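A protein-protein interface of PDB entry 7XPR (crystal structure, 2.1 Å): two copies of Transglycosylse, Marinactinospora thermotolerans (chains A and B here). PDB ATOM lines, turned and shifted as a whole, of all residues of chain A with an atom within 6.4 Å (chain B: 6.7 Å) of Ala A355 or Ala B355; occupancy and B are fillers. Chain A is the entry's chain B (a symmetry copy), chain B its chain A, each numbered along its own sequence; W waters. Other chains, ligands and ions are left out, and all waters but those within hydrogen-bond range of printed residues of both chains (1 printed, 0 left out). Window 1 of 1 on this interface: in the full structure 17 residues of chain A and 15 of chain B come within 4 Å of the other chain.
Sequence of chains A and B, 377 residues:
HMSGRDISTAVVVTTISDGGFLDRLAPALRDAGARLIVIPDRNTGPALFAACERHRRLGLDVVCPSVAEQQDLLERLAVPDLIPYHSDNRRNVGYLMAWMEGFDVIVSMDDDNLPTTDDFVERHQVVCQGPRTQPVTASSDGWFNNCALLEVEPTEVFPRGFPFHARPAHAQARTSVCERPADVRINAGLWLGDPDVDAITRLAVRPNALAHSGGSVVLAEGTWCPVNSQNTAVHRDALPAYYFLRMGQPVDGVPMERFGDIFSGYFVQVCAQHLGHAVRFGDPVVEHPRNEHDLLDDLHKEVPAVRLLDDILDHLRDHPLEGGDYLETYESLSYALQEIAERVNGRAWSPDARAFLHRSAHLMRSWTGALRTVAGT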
ATOM      1  N   GLN A 249     -22.827  16.226   5.089  1.00  0.00           N
ATOM      2  CA  GLN A 249     -23.541  15.872   6.311  1.00  0.00           C
ATOM      3  C   GLN A 249     -23.738  17.110   7.177  1.00  0.00           C
ATOM      4  O   GLN A 249     -22.768  17.825   7.459  1.00  0.00           O
ATOM      5  CB  GLN A 249     -22.779  14.800   7.088  1.00  0.00           C
ATOM      6  CG  GLN A 249     -22.851  13.416   6.467  1.00  0.00           C
ATOM      7  CD  GLN A 249     -24.251  12.835   6.505  1.00  0.00           C
ATOM      8  OE1 GLN A 249     -24.681  12.164   5.568  1.00  0.00           O
ATOM      9  NE2 GLN A 249     -24.967  13.089   7.594  1.00  0.00           N
ATOM     10  N   ALA A 341     -18.604   8.301  18.320  1.00  0.00           N
ATOM     11  CA  ALA A 341     -19.777   9.128  18.057  1.00  0.00           C
ATOM     12  C   ALA A 341     -20.778   9.112  19.205  1.00  0.00           C
ATOM     13  O   ALA A 341     -21.568  10.053  19.334  1.00  0.00           O
ATOM     14  CB  ALA A 341     -20.460   8.672  16.767  1.00  0.00           C
ATOM     15  N   GLU A 342     -20.764   8.072  20.039  1.00  0.00           N
ATOM     16  CA  GLU A 342     -21.672   7.988  21.174  1.00  0.00           C
ATOM     17  C   GLU A 342     -21.007   8.318  22.504  1.00  0.00           C
ATOM     18  O   GLU A 342     -21.713   8.634  23.467  1.00  0.00           O
ATOM     19  CB  GLU A 342     -22.293   6.587  21.255  1.00  0.00           C
ATOM     20  CG  GLU A 342     -22.977   6.139  19.972  1.00  0.00           C
ATOM     21  CD  GLU A 342     -24.100   7.068  19.552  1.00  0.00           C
ATOM     22  OE1 GLU A 342     -24.825   7.569  20.437  1.00  0.00           O
ATOM     23  OE2 GLU A 342     -24.257   7.301  18.334  1.00  0.00           O
ATOM     24  N   SER A 350     -24.622  17.529  18.400  1.00  0.00           N
ATOM     25  CA  SER A 350     -26.048  17.321  18.246  1.00  0.00           C
ATOM     26  C   SER A 350     -26.293  15.935  17.651  1.00  0.00           C
ATOM     27  O   SER A 350     -25.351  15.253  17.241  1.00  0.00           O
ATOM     28  CB  SER A 350     -26.636  18.425  17.365  1.00  0.00           C
ATOM     29  OG  SER A 350     -25.939  18.520  16.137  1.00  0.00           O
ATOM     30  N   PRO A 351     -27.551  15.475  17.612  1.00  0.00           N
ATOM     31  CA  PRO A 351     -27.817  14.156  17.006  1.00  0.00           C
ATOM     32  C   PRO A 351     -27.321  14.021  15.574  1.00  0.00           C
ATOM     33  O   PRO A 351     -26.866  12.937  15.187  1.00  0.00           O
ATOM     34  CB  PRO A 351     -29.342  14.040  17.097  1.00  0.00           C
ATOM     35  CG  PRO A 351     -29.693  14.826  18.304  1.00  0.00           C
ATOM     36  CD  PRO A 351     -28.737  15.990  18.326  1.00  0.00           C
ATOM     37  N   ASP A 352     -27.393  15.086  14.771  1.00  0.00           N
ATOM     38  CA  ASP A 352     -26.939  14.976  13.387  1.00  0.00           C
ATOM     39  C   ASP A 352     -25.420  14.924  13.295  1.00  0.00           C
ATOM     40  O   ASP A 352     -24.879  14.323  12.359  1.00  0.00           O
ATOM     41  CB  ASP A 352     -27.489  16.133  12.549  1.00  0.00           C
ATOM     42  CG  ASP A 352     -27.084  17.495  13.081  1.00  0.00           C
ATOM     43  OD1 ASP A 352     -26.447  17.561  14.155  1.00  0.00           O
ATOM     44  OD2 ASP A 352     -27.402  18.505  12.419  1.00  0.00           O
ATOM     45  N   ALA A 353     -24.717  15.543  14.246  1.00  0.00           N
ATOM     46  CA  ALA A 353     -23.261  15.456  14.259  1.00  0.00           C
ATOM     47  C   ALA A 353     -22.798  14.046  14.598  1.00  0.00           C
ATOM     48  O   ALA A 353     -21.838  13.541  14.004  1.00  0.00           O
ATOM     49  CB  ALA A 353     -22.679  16.467  15.246  1.00  0.00           C
ATOM     50  N   ARG A 354     -23.467  13.395  15.554  1.00  0.00           N
ATOM     51  CA  ARG A 354     -23.135  12.011  15.874  1.00  0.00           C
ATOM     52  C   ARG A 354     -23.445  11.087  14.703  1.00  0.00           C
ATOM     53  O   ARG A 354     -22.647  10.199  14.377  1.00  0.00           O
ATOM     54  CB  ARG A 354     -23.897  11.559  17.120  1.00  0.00           C
ATOM     55  CG  ARG A 354     -23.666  12.424  18.348  1.00  0.00           C
ATOM     56  CD  ARG A 354     -24.365  11.835  19.564  1.00  0.00           C
ATOM     57  NE  ARG A 354     -24.226  12.682  20.742  1.00  0.00           N
ATOM     58  CZ  ARG A 354     -23.194  12.645  21.574  1.00  0.00           C
ATOM     59  NH1 ARG A 354     -22.182  11.812  21.385  1.00  0.00           N
ATOM     60  NH2 ARG A 354     -23.175  13.463  22.622  1.00  0.00           N
ATOM     61  N   ALA A 355     -24.597  11.283  14.058  1.00  0.00           N
ATOM     62  CA  ALA A 355     -24.980  10.444  12.928  1.00  0.00           C
ATOM     63  C   ALA A 355     -24.068  10.641  11.724  1.00  0.00           C
ATOM     64  O   ALA A 355     -24.004   9.759  10.862  1.00  0.00           O
ATOM     65  CB  ALA A 355     -26.430  10.721  12.536  1.00  0.00           C
ATOM     66  N   PHE A 356     -23.368  11.777  11.645  1.00  0.00           N
ATOM     67  CA  PHE A 356     -22.403  11.977  10.569  1.00  0.00           C
ATOM     68  C   PHE A 356     -21.294  10.936  10.627  1.00  0.00           C
ATOM     69  O   PHE A 356     -20.878  10.401   9.593  1.00  0.00           O
ATOM     70  CB  PHE A 356     -21.828  13.394  10.642  1.00  0.00           C
ATOM     71  CG  PHE A 356     -20.376  13.485  10.257  1.00  0.00           C
ATOM     72  CD1 PHE A 356     -19.992  13.456   8.926  1.00  0.00           C
ATOM     73  CD2 PHE A 356     -19.397  13.612  11.228  1.00  0.00           C
ATOM     74  CE1 PHE A 356     -18.658  13.539   8.571  1.00  0.00           C
ATOM     75  CE2 PHE A 356     -18.061  13.699  10.880  1.00  0.00           C
ATOM     76  CZ  PHE A 356     -17.691  13.663   9.549  1.00  0.00           C
ATOM     77  N   LEU A 357     -20.800  10.631  11.831  1.00  0.00           N
ATOM     78  CA  LEU A 357     -19.773   9.603  11.965  1.00  0.00           C
ATOM     79  C   LEU A 357     -20.323   8.218  11.647  1.00  0.00           C
ATOM     80  O   LEU A 357     -19.584   7.362  11.147  1.00  0.00           O
ATOM     81  CB  LEU A 357     -19.179   9.628  13.373  1.00  0.00           C
ATOM     82  CG  LEU A 357     -18.264  10.808  13.714  1.00  0.00           C
ATOM     83  CD1 LEU A 357     -17.806  10.735  15.163  1.00  0.00           C
ATOM     84  CD2 LEU A 357     -17.066  10.845  12.777  1.00  0.00           C
ATOM     85  N   HIS A 358     -21.605   7.979  11.925  1.00  0.00           N
ATOM     86  CA  HIS A 358     -22.186   6.671  11.646  1.00  0.00           C
ATOM     87  C   HIS A 358     -22.397   6.463  10.151  1.00  0.00           C
ATOM     88  O   HIS A 358     -22.127   5.376   9.627  1.00  0.00           O
ATOM     89  CB  HIS A 358     -23.502   6.505  12.407  1.00  0.00           C
ATOM     90  CG  HIS A 358     -23.332   6.417  13.891  1.00  0.00           C
ATOM     91  ND1 HIS A 358     -22.774   5.321  14.512  1.00  0.00           N
ATOM     92  CD2 HIS A 358     -23.647   7.290  14.879  1.00  0.00           C
ATOM     93  CE1 HIS A 358     -22.752   5.521  15.818  1.00  0.00           C
ATOM     94  NE2 HIS A 358     -23.276   6.707  16.066  1.00  0.00           N
ATOM     95  N   ARG A 359     -22.880   7.489   9.446  1.00  0.00           N
ATOM     96  CA  ARG A 359     -23.026   7.370   7.999  1.00  0.00           C
ATOM     97  C   ARG A 359     -21.666   7.279   7.319  1.00  0.00           C
ATOM     98  O   ARG A 359     -21.489   6.500   6.375  1.00  0.00           O
ATOM     99  CB  ARG A 359     -23.830   8.545   7.443  1.00  0.00           C
ATOM    100  CG  ARG A 359     -23.922   8.554   5.924  1.00  0.00           C
ATOM    101  CD  ARG A 359     -25.301   8.981   5.445  1.00  0.00           C
ATOM    102  NE  ARG A 359     -25.460   8.786   4.008  1.00  0.00           N
ATOM    103  CZ  ARG A 359     -25.356   9.750   3.102  1.00  0.00           C
ATOM    104  NH1 ARG A 359     -25.109  11.002   3.450  1.00  0.00           N
ATOM    105  NH2 ARG A 359     -25.506   9.448   1.816  1.00  0.00           N
ATOM    106  N   SER A 360     -20.693   8.065   7.786  1.00  0.00           N
ATOM    107  CA  SER A 360     -19.337   7.957   7.256  1.00  0.00           C
ATOM    108  C   SER A 360     -18.757   6.570   7.497  1.00  0.00           C
ATOM    109  O   SER A 360     -17.975   6.076   6.678  1.00  0.00           O
ATOM    110  CB  SER A 360     -18.438   9.024   7.881  1.00  0.00           C
ATOM    111  OG  SER A 360     -18.893  10.327   7.568  1.00  0.00           O
ATOM    112  N   GLN B 249     -33.556  12.228  16.122  1.00  0.00           N
ATOM    113  CA  GLN B 249     -32.761  12.428  14.916  1.00  0.00           C
ATOM    114  C   GLN B 249     -33.465  13.410  13.986  1.00  0.00           C
ATOM    115  O   GLN B 249     -34.666  13.264  13.732  1.00  0.00           O
ATOM    116  CB  GLN B 249     -32.526  11.100  14.201  1.00  0.00           C
ATOM    117  CG  GLN B 249     -31.560  10.174  14.918  1.00  0.00           C
ATOM    118  CD  GLN B 249     -30.154  10.735  14.975  1.00  0.00           C
ATOM    119  OE1 GLN B 249     -29.464  10.612  15.987  1.00  0.00           O
ATOM    120  NE2 GLN B 249     -29.718  11.355  13.884  1.00  0.00           N
ATOM    121  N   PRO B 250     -32.765  14.414  13.466  1.00  0.00           N
ATOM    122  CA  PRO B 250     -33.415  15.381  12.576  1.00  0.00           C
ATOM    123  C   PRO B 250     -33.647  14.810  11.185  1.00  0.00           C
ATOM    124  O   PRO B 250     -32.848  14.027  10.665  1.00  0.00           O
ATOM    125  CB  PRO B 250     -32.418  16.546  12.537  1.00  0.00           C
ATOM    126  CG  PRO B 250     -31.100  15.900  12.774  1.00  0.00           C
ATOM    127  CD  PRO B 250     -31.360  14.766  13.733  1.00  0.00           C
ATOM    128  N   ALA B 341     -30.657   2.836   3.520  1.00  0.00           N
ATOM    129  CA  ALA B 341     -30.413   4.263   3.694  1.00  0.00           C
ATOM    130  C   ALA B 341     -29.659   4.877   2.522  1.00  0.00           C
ATOM    131  O   ALA B 341     -29.715   6.098   2.336  1.00  0.00           O
ATOM    132  CB  ALA B 341     -29.643   4.508   4.992  1.00  0.00           C
ATOM    133  N   GLU B 342     -28.957   4.066   1.729  1.00  0.00           N
ATOM    134  CA  GLU B 342     -28.216   4.571   0.581  1.00  0.00           C
ATOM    135  C   GLU B 342     -28.906   4.308  -0.751  1.00  0.00           C
ATOM    136  O   GLU B 342     -28.642   5.031  -1.718  1.00  0.00           O
ATOM    137  CB  GLU B 342     -26.808   3.962   0.547  1.00  0.00           C
ATOM    138  CG  GLU B 342     -25.991   4.231   1.801  1.00  0.00           C
ATOM    139  CD  GLU B 342     -25.806   5.713   2.069  1.00  0.00           C
ATOM    140  OE1 GLU B 342     -25.604   6.474   1.100  1.00  0.00           O
ATOM    141  OE2 GLU B 342     -25.871   6.117   3.250  1.00  0.00           O
ATOM    142  N   TRP B 349     -35.371  12.490   1.631  1.00  0.00           N
ATOM    143  CA  TRP B 349     -34.166  11.754   2.011  1.00  0.00           C
ATOM    144  C   TRP B 349     -32.936  12.649   1.859  1.00  0.00           C
ATOM    145  O   TRP B 349     -32.095  12.485   0.974  1.00  0.00           O
ATOM    146  CB  TRP B 349     -34.051  10.471   1.196  1.00  0.00           C
ATOM    147  CG  TRP B 349     -35.048   9.443   1.627  1.00  0.00           C
ATOM    148  CD1 TRP B 349     -36.220   9.125   1.008  1.00  0.00           C
ATOM    149  CD2 TRP B 349     -34.972   8.617   2.795  1.00  0.00           C
ATOM    150  NE1 TRP B 349     -36.875   8.142   1.711  1.00  0.00           N
ATOM    151  CE2 TRP B 349     -36.128   7.812   2.812  1.00  0.00           C
ATOM    152  CE3 TRP B 349     -34.035   8.473   3.824  1.00  0.00           C
ATOM    153  CZ2 TRP B 349     -36.374   6.878   3.818  1.00  0.00           C
ATOM    154  CZ3 TRP B 349     -34.279   7.545   4.821  1.00  0.00           C
ATOM    155  CH2 TRP B 349     -35.439   6.760   4.811  1.00  0.00           C
ATOM    156  N   SER B 350     -32.854  13.616   2.766  1.00  0.00           N
ATOM    157  CA  SER B 350     -31.690  14.473   2.897  1.00  0.00           C
ATOM    158  C   SER B 350     -30.561  13.696   3.566  1.00  0.00           C
ATOM    159  O   SER B 350     -30.766  12.583   4.051  1.00  0.00           O
ATOM    160  CB  SER B 350     -32.070  15.721   3.693  1.00  0.00           C
ATOM    161  OG  SER B 350     -32.654  15.375   4.936  1.00  0.00           O
ATOM    162  N   PRO B 351     -29.340  14.247   3.583  1.00  0.00           N
ATOM    163  CA  PRO B 351     -28.237  13.528   4.246  1.00  0.00           C
ATOM    164  C   PRO B 351     -28.511  13.168   5.698  1.00  0.00           C
ATOM    165  O   PRO B 351     -28.100  12.090   6.147  1.00  0.00           O
ATOM    166  CB  PRO B 351     -27.063  14.506   4.112  1.00  0.00           C
ATOM    167  CG  PRO B 351     -27.348  15.234   2.851  1.00  0.00           C
ATOM    168  CD  PRO B 351     -28.845  15.396   2.800  1.00  0.00           C
ATOM    169  N   ASP B 352     -29.199  14.031   6.450  1.00  0.00           N
ATOM    170  CA  ASP B 352     -29.465  13.713   7.851  1.00  0.00           C
ATOM    171  C   ASP B 352     -30.517  12.621   7.992  1.00  0.00           C
ATOM    172  O   ASP B 352     -30.489  11.859   8.965  1.00  0.00           O
ATOM    173  CB  ASP B 352     -29.885  14.970   8.616  1.00  0.00           C
ATOM    174  CG  ASP B 352     -31.151  15.605   8.067  1.00  0.00           C
ATOM    175  OD1 ASP B 352     -31.656  15.149   7.019  1.00  0.00           O
ATOM    176  OD2 ASP B 352     -31.642  16.570   8.690  1.00  0.00           O
ATOM    177  N   ALA B 353     -31.448  12.526   7.039  1.00  0.00           N
ATOM    178  CA  ALA B 353     -32.431  11.449   7.075  1.00  0.00           C
ATOM    179  C   ALA B 353     -31.774  10.098   6.819  1.00  0.00           C
ATOM    180  O   ALA B 353     -32.120   9.101   7.463  1.00  0.00           O
ATOM    181  CB  ALA B 353     -33.539  11.710   6.056  1.00  0.00           C
ATOM    182  N   ARG B 354     -30.826  10.047   5.880  1.00  0.00           N
ATOM    183  CA  ARG B 354     -30.089   8.811   5.642  1.00  0.00           C
ATOM    184  C   ARG B 354     -29.228   8.445   6.844  1.00  0.00           C
ATOM    185  O   ARG B 354     -29.153   7.272   7.229  1.00  0.00           O
ATOM    186  CB  ARG B 354     -29.222   8.944   4.390  1.00  0.00           C
ATOM    187  CG  ARG B 354     -29.987   9.312   3.132  1.00  0.00           C
ATOM    188  CD  ARG B 354     -29.060   9.370   1.929  1.00  0.00           C
ATOM    189  NE  ARG B 354     -29.766   9.749   0.712  1.00  0.00           N
ATOM    190  CZ  ARG B 354     -30.403   8.899  -0.082  1.00  0.00           C
ATOM    191  NH1 ARG B 354     -30.447   7.605   0.187  1.00  0.00           N
ATOM    192  NH2 ARG B 354     -31.011   9.359  -1.171  1.00  0.00           N
ATOM    193  N   ALA B 355     -28.572   9.438   7.450  1.00  0.00           N
ATOM    194  CA  ALA B 355     -27.735   9.183   8.616  1.00  0.00           C
ATOM    195  C   ALA B 355     -28.546   8.755   9.831  1.00  0.00           C
ATOM    196  O   ALA B 355     -27.981   8.170  10.762  1.00  0.00           O
ATOM    197  CB  ALA B 355     -26.910  10.426   8.949  1.00  0.00           C
ATOM    198  N   PHE B 356     -29.852   9.038   9.848  1.00  0.00           N
ATOM    199  CA  PHE B 356     -30.699   8.557  10.934  1.00  0.00           C
ATOM    200  C   PHE B 356     -30.743   7.035  10.966  1.00  0.00           C
ATOM    201  O   PHE B 356     -30.659   6.426  12.039  1.00  0.00           O
ATOM    202  CB  PHE B 356     -32.109   9.137  10.796  1.00  0.00           C
ATOM    203  CG  PHE B 356     -33.199   8.200  11.238  1.00  0.00           C
ATOM    204  CD1 PHE B 356     -33.440   7.977  12.584  1.00  0.00           C
ATOM    205  CD2 PHE B 356     -33.992   7.550  10.305  1.00  0.00           C
ATOM    206  CE1 PHE B 356     -34.442   7.114  12.991  1.00  0.00           C
ATOM    207  CE2 PHE B 356     -34.997   6.689  10.706  1.00  0.00           C
ATOM    208  CZ  PHE B 356     -35.223   6.471  12.049  1.00  0.00           C
ATOM    209  N   LEU B 357     -30.875   6.402   9.797  1.00  0.00           N
ATOM    210  CA  LEU B 357     -30.891   4.943   9.750  1.00  0.00           C
ATOM    211  C   LEU B 357     -29.538   4.352  10.124  1.00  0.00           C
ATOM    212  O   LEU B 357     -29.480   3.264  10.708  1.00  0.00           O
ATOM    213  CB  LEU B 357     -31.312   4.463   8.360  1.00  0.00           C
ATOM    214  CG  LEU B 357     -32.791   4.623   8.000  1.00  0.00           C
ATOM    215  CD1 LEU B 357     -33.051   4.159   6.574  1.00  0.00           C
ATOM    216  CD2 LEU B 357     -33.665   3.858   8.980  1.00  0.00           C
ATOM    217  N   HIS B 358     -28.446   5.048   9.801  1.00  0.00           N
ATOM    218  CA  HIS B 358     -27.122   4.533  10.136  1.00  0.00           C
ATOM    219  C   HIS B 358     -26.868   4.591  11.638  1.00  0.00           C
ATOM    220  O   HIS B 358     -26.337   3.638  12.219  1.00  0.00           O
ATOM    221  CB  HIS B 358     -26.048   5.308   9.373  1.00  0.00           C
ATOM    222  CG  HIS B 358     -26.084   5.090   7.892  1.00  0.00           C
ATOM    223  ND1 HIS B 358     -25.753   3.884   7.309  1.00  0.00           N
ATOM    224  CD2 HIS B 358     -26.411   5.921   6.874  1.00  0.00           C
ATOM    225  CE1 HIS B 358     -25.876   3.983   5.997  1.00  0.00           C
ATOM    226  NE2 HIS B 358     -26.273   5.209   5.707  1.00  0.00           N
ATOM    227  N   ARG B 359     -27.239   5.698  12.285  1.00  0.00           N
ATOM    228  CA  ARG B 359     -27.064   5.787  13.731  1.00  0.00           C
ATOM    229  C   ARG B 359     -28.000   4.831  14.458  1.00  0.00           C
ATOM    230  O   ARG B 359     -27.618   4.224  15.465  1.00  0.00           O
ATOM    231  CB  ARG B 359     -27.282   7.223  14.208  1.00  0.00           C
ATOM    232  CG  ARG B 359     -27.145   7.396  15.716  1.00  0.00           C
ATOM    233  CD  ARG B 359     -26.782   8.825  16.089  1.00  0.00           C
ATOM    234  NE  ARG B 359     -26.474   8.955  17.509  1.00  0.00           N
ATOM    235  CZ  ARG B 359     -27.283   9.495  18.409  1.00  0.00           C
ATOM    236  NH1 ARG B 359     -28.461   9.992  18.071  1.00  0.00           N
ATOM    237  NH2 ARG B 359     -26.900   9.542  19.683  1.00  0.00           N
ATOM    238  N   SER B 360     -29.230   4.680  13.958  1.00  0.00           N
ATOM    239  CA  SER B 360     -30.162   3.733  14.562  1.00  0.00           C
ATOM    240  C   SER B 360     -29.624   2.310  14.491  1.00  0.00           C
ATOM    241  O   SER B 360     -29.780   1.532  15.439  1.00  0.00           O
ATOM    242  CB  SER B 360     -31.524   3.826  13.873  1.00  0.00           C
ATOM    243  OG  SER B 360     -32.079   5.122  14.005  1.00  0.00           O
HETATM  244  O   HOH W   1     -29.921  18.610  10.392  1.00  0.00           O
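Of the printed residues of chain B, Asp A352 touches Pro B250 (3.6 Å).
Printed residues of chain B within 4 Å of Arg A354: Arg B359 (3.4 Å).
Of the printed residues of chain A, Gln B249 touches Pro A351 and Ala A355.
Of chain A, only Gln A249, Ala A355 and Arg A359 come within 4 Å of Ala B355.
The nearest residue of chain B that does not touch Ala A355 is Phe B356 (4.7 Å).
Of the 14 printed residues of chain A, 8 touch a printed residue of chain B.
Among the printed residues, 16 pairs touch across the chains.
Among the printed residues, Asp or Glu carboxylates within 4 Å of a Lys or Arg side-chain nitrogen of the other chain: Glu A342 with Arg B359 (2.9 Å) and Arg A359 with Glu B342 (2.8 Å).
Pro B250 touches Pro A351.
CB of Asp A352 touches CG of Pro B250, 3.6 Å away.
Ala A355 touches Gln B249.
CB of Ala A355 touches O of Ala B355, 3.5 Å away.
CD of Arg B359 touches N of Ala A355 (3.9 Å).
His B358 touches His A358.
Arg B359 touches His A358.
CD of Arg B354 touches NH2 of Arg A359, 3.6 Å away.
CD of Arg A359 touches N of Ala B355, at 3.9 Å.
His B358 touches Arg A359 (CD2 to CD, 3.6 Å).
Water W1 bridges OD2 of Asp B352 (3.2 Å) and OD2 of Asp A352 (3.2 Å).
Gln A249 touches Ala B355, and with the chains exchanged Ala A355 touches Gln B249.
Ala A355 touches Arg B359, and with the chains exchanged Arg A359 touches Ala B355.
His A358 touches its own counterpart, His B358.
His A358 touches Arg B359, and with the chains exchanged Arg A359 touches His B358.
Positions printed for both chains: 249, 341, 342, 350, 351, 352, 353, 354, 355, 356, 357, 358, 359 and 360.
Of the 16 pairs that touch across the chains among the printed residues, 14 have their exchanged pair printed and touching as well.
The guanidinium group of Arg A359 lies within salt-bridge range of the side-chain carboxylate of Glu B342 (2.8 Å).
The backbone carbonyl oxygen (O) of Pro B351 lies close to the side-chain amide oxygen (OE1) of Gln A249, 3.5 Å away.
The guanidinium group (NE) of Arg B359 is in salt-bridge range of the side-chain carboxylate (OE2) of Glu A342 (2.9 Å).
The backbone carbonyl oxygen of Ala B341 is in hydrogen-bond range of the guanidinium group of Arg B354, at 2.7 Å.
The side-chain carboxylate (OE2) of Glu B342 is in hydrogen-bond range of a ring nitrogen (NE2) of His B358 (2.7 Å).
The side-chain amide oxygen of Gln A249 sits at hydrogen-bond distance from the guanidinium group of Arg A359, 2.5 Å away.
NH1 of Arg A354 sits at hydrogen-bond distance from O of Ala A341, at 2.8 Å.
The side-chain carboxylate (OE2) of Glu A342 lies within hydrogen-bond range of a ring nitrogen (NE2) of His A358 (2.5 Å).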
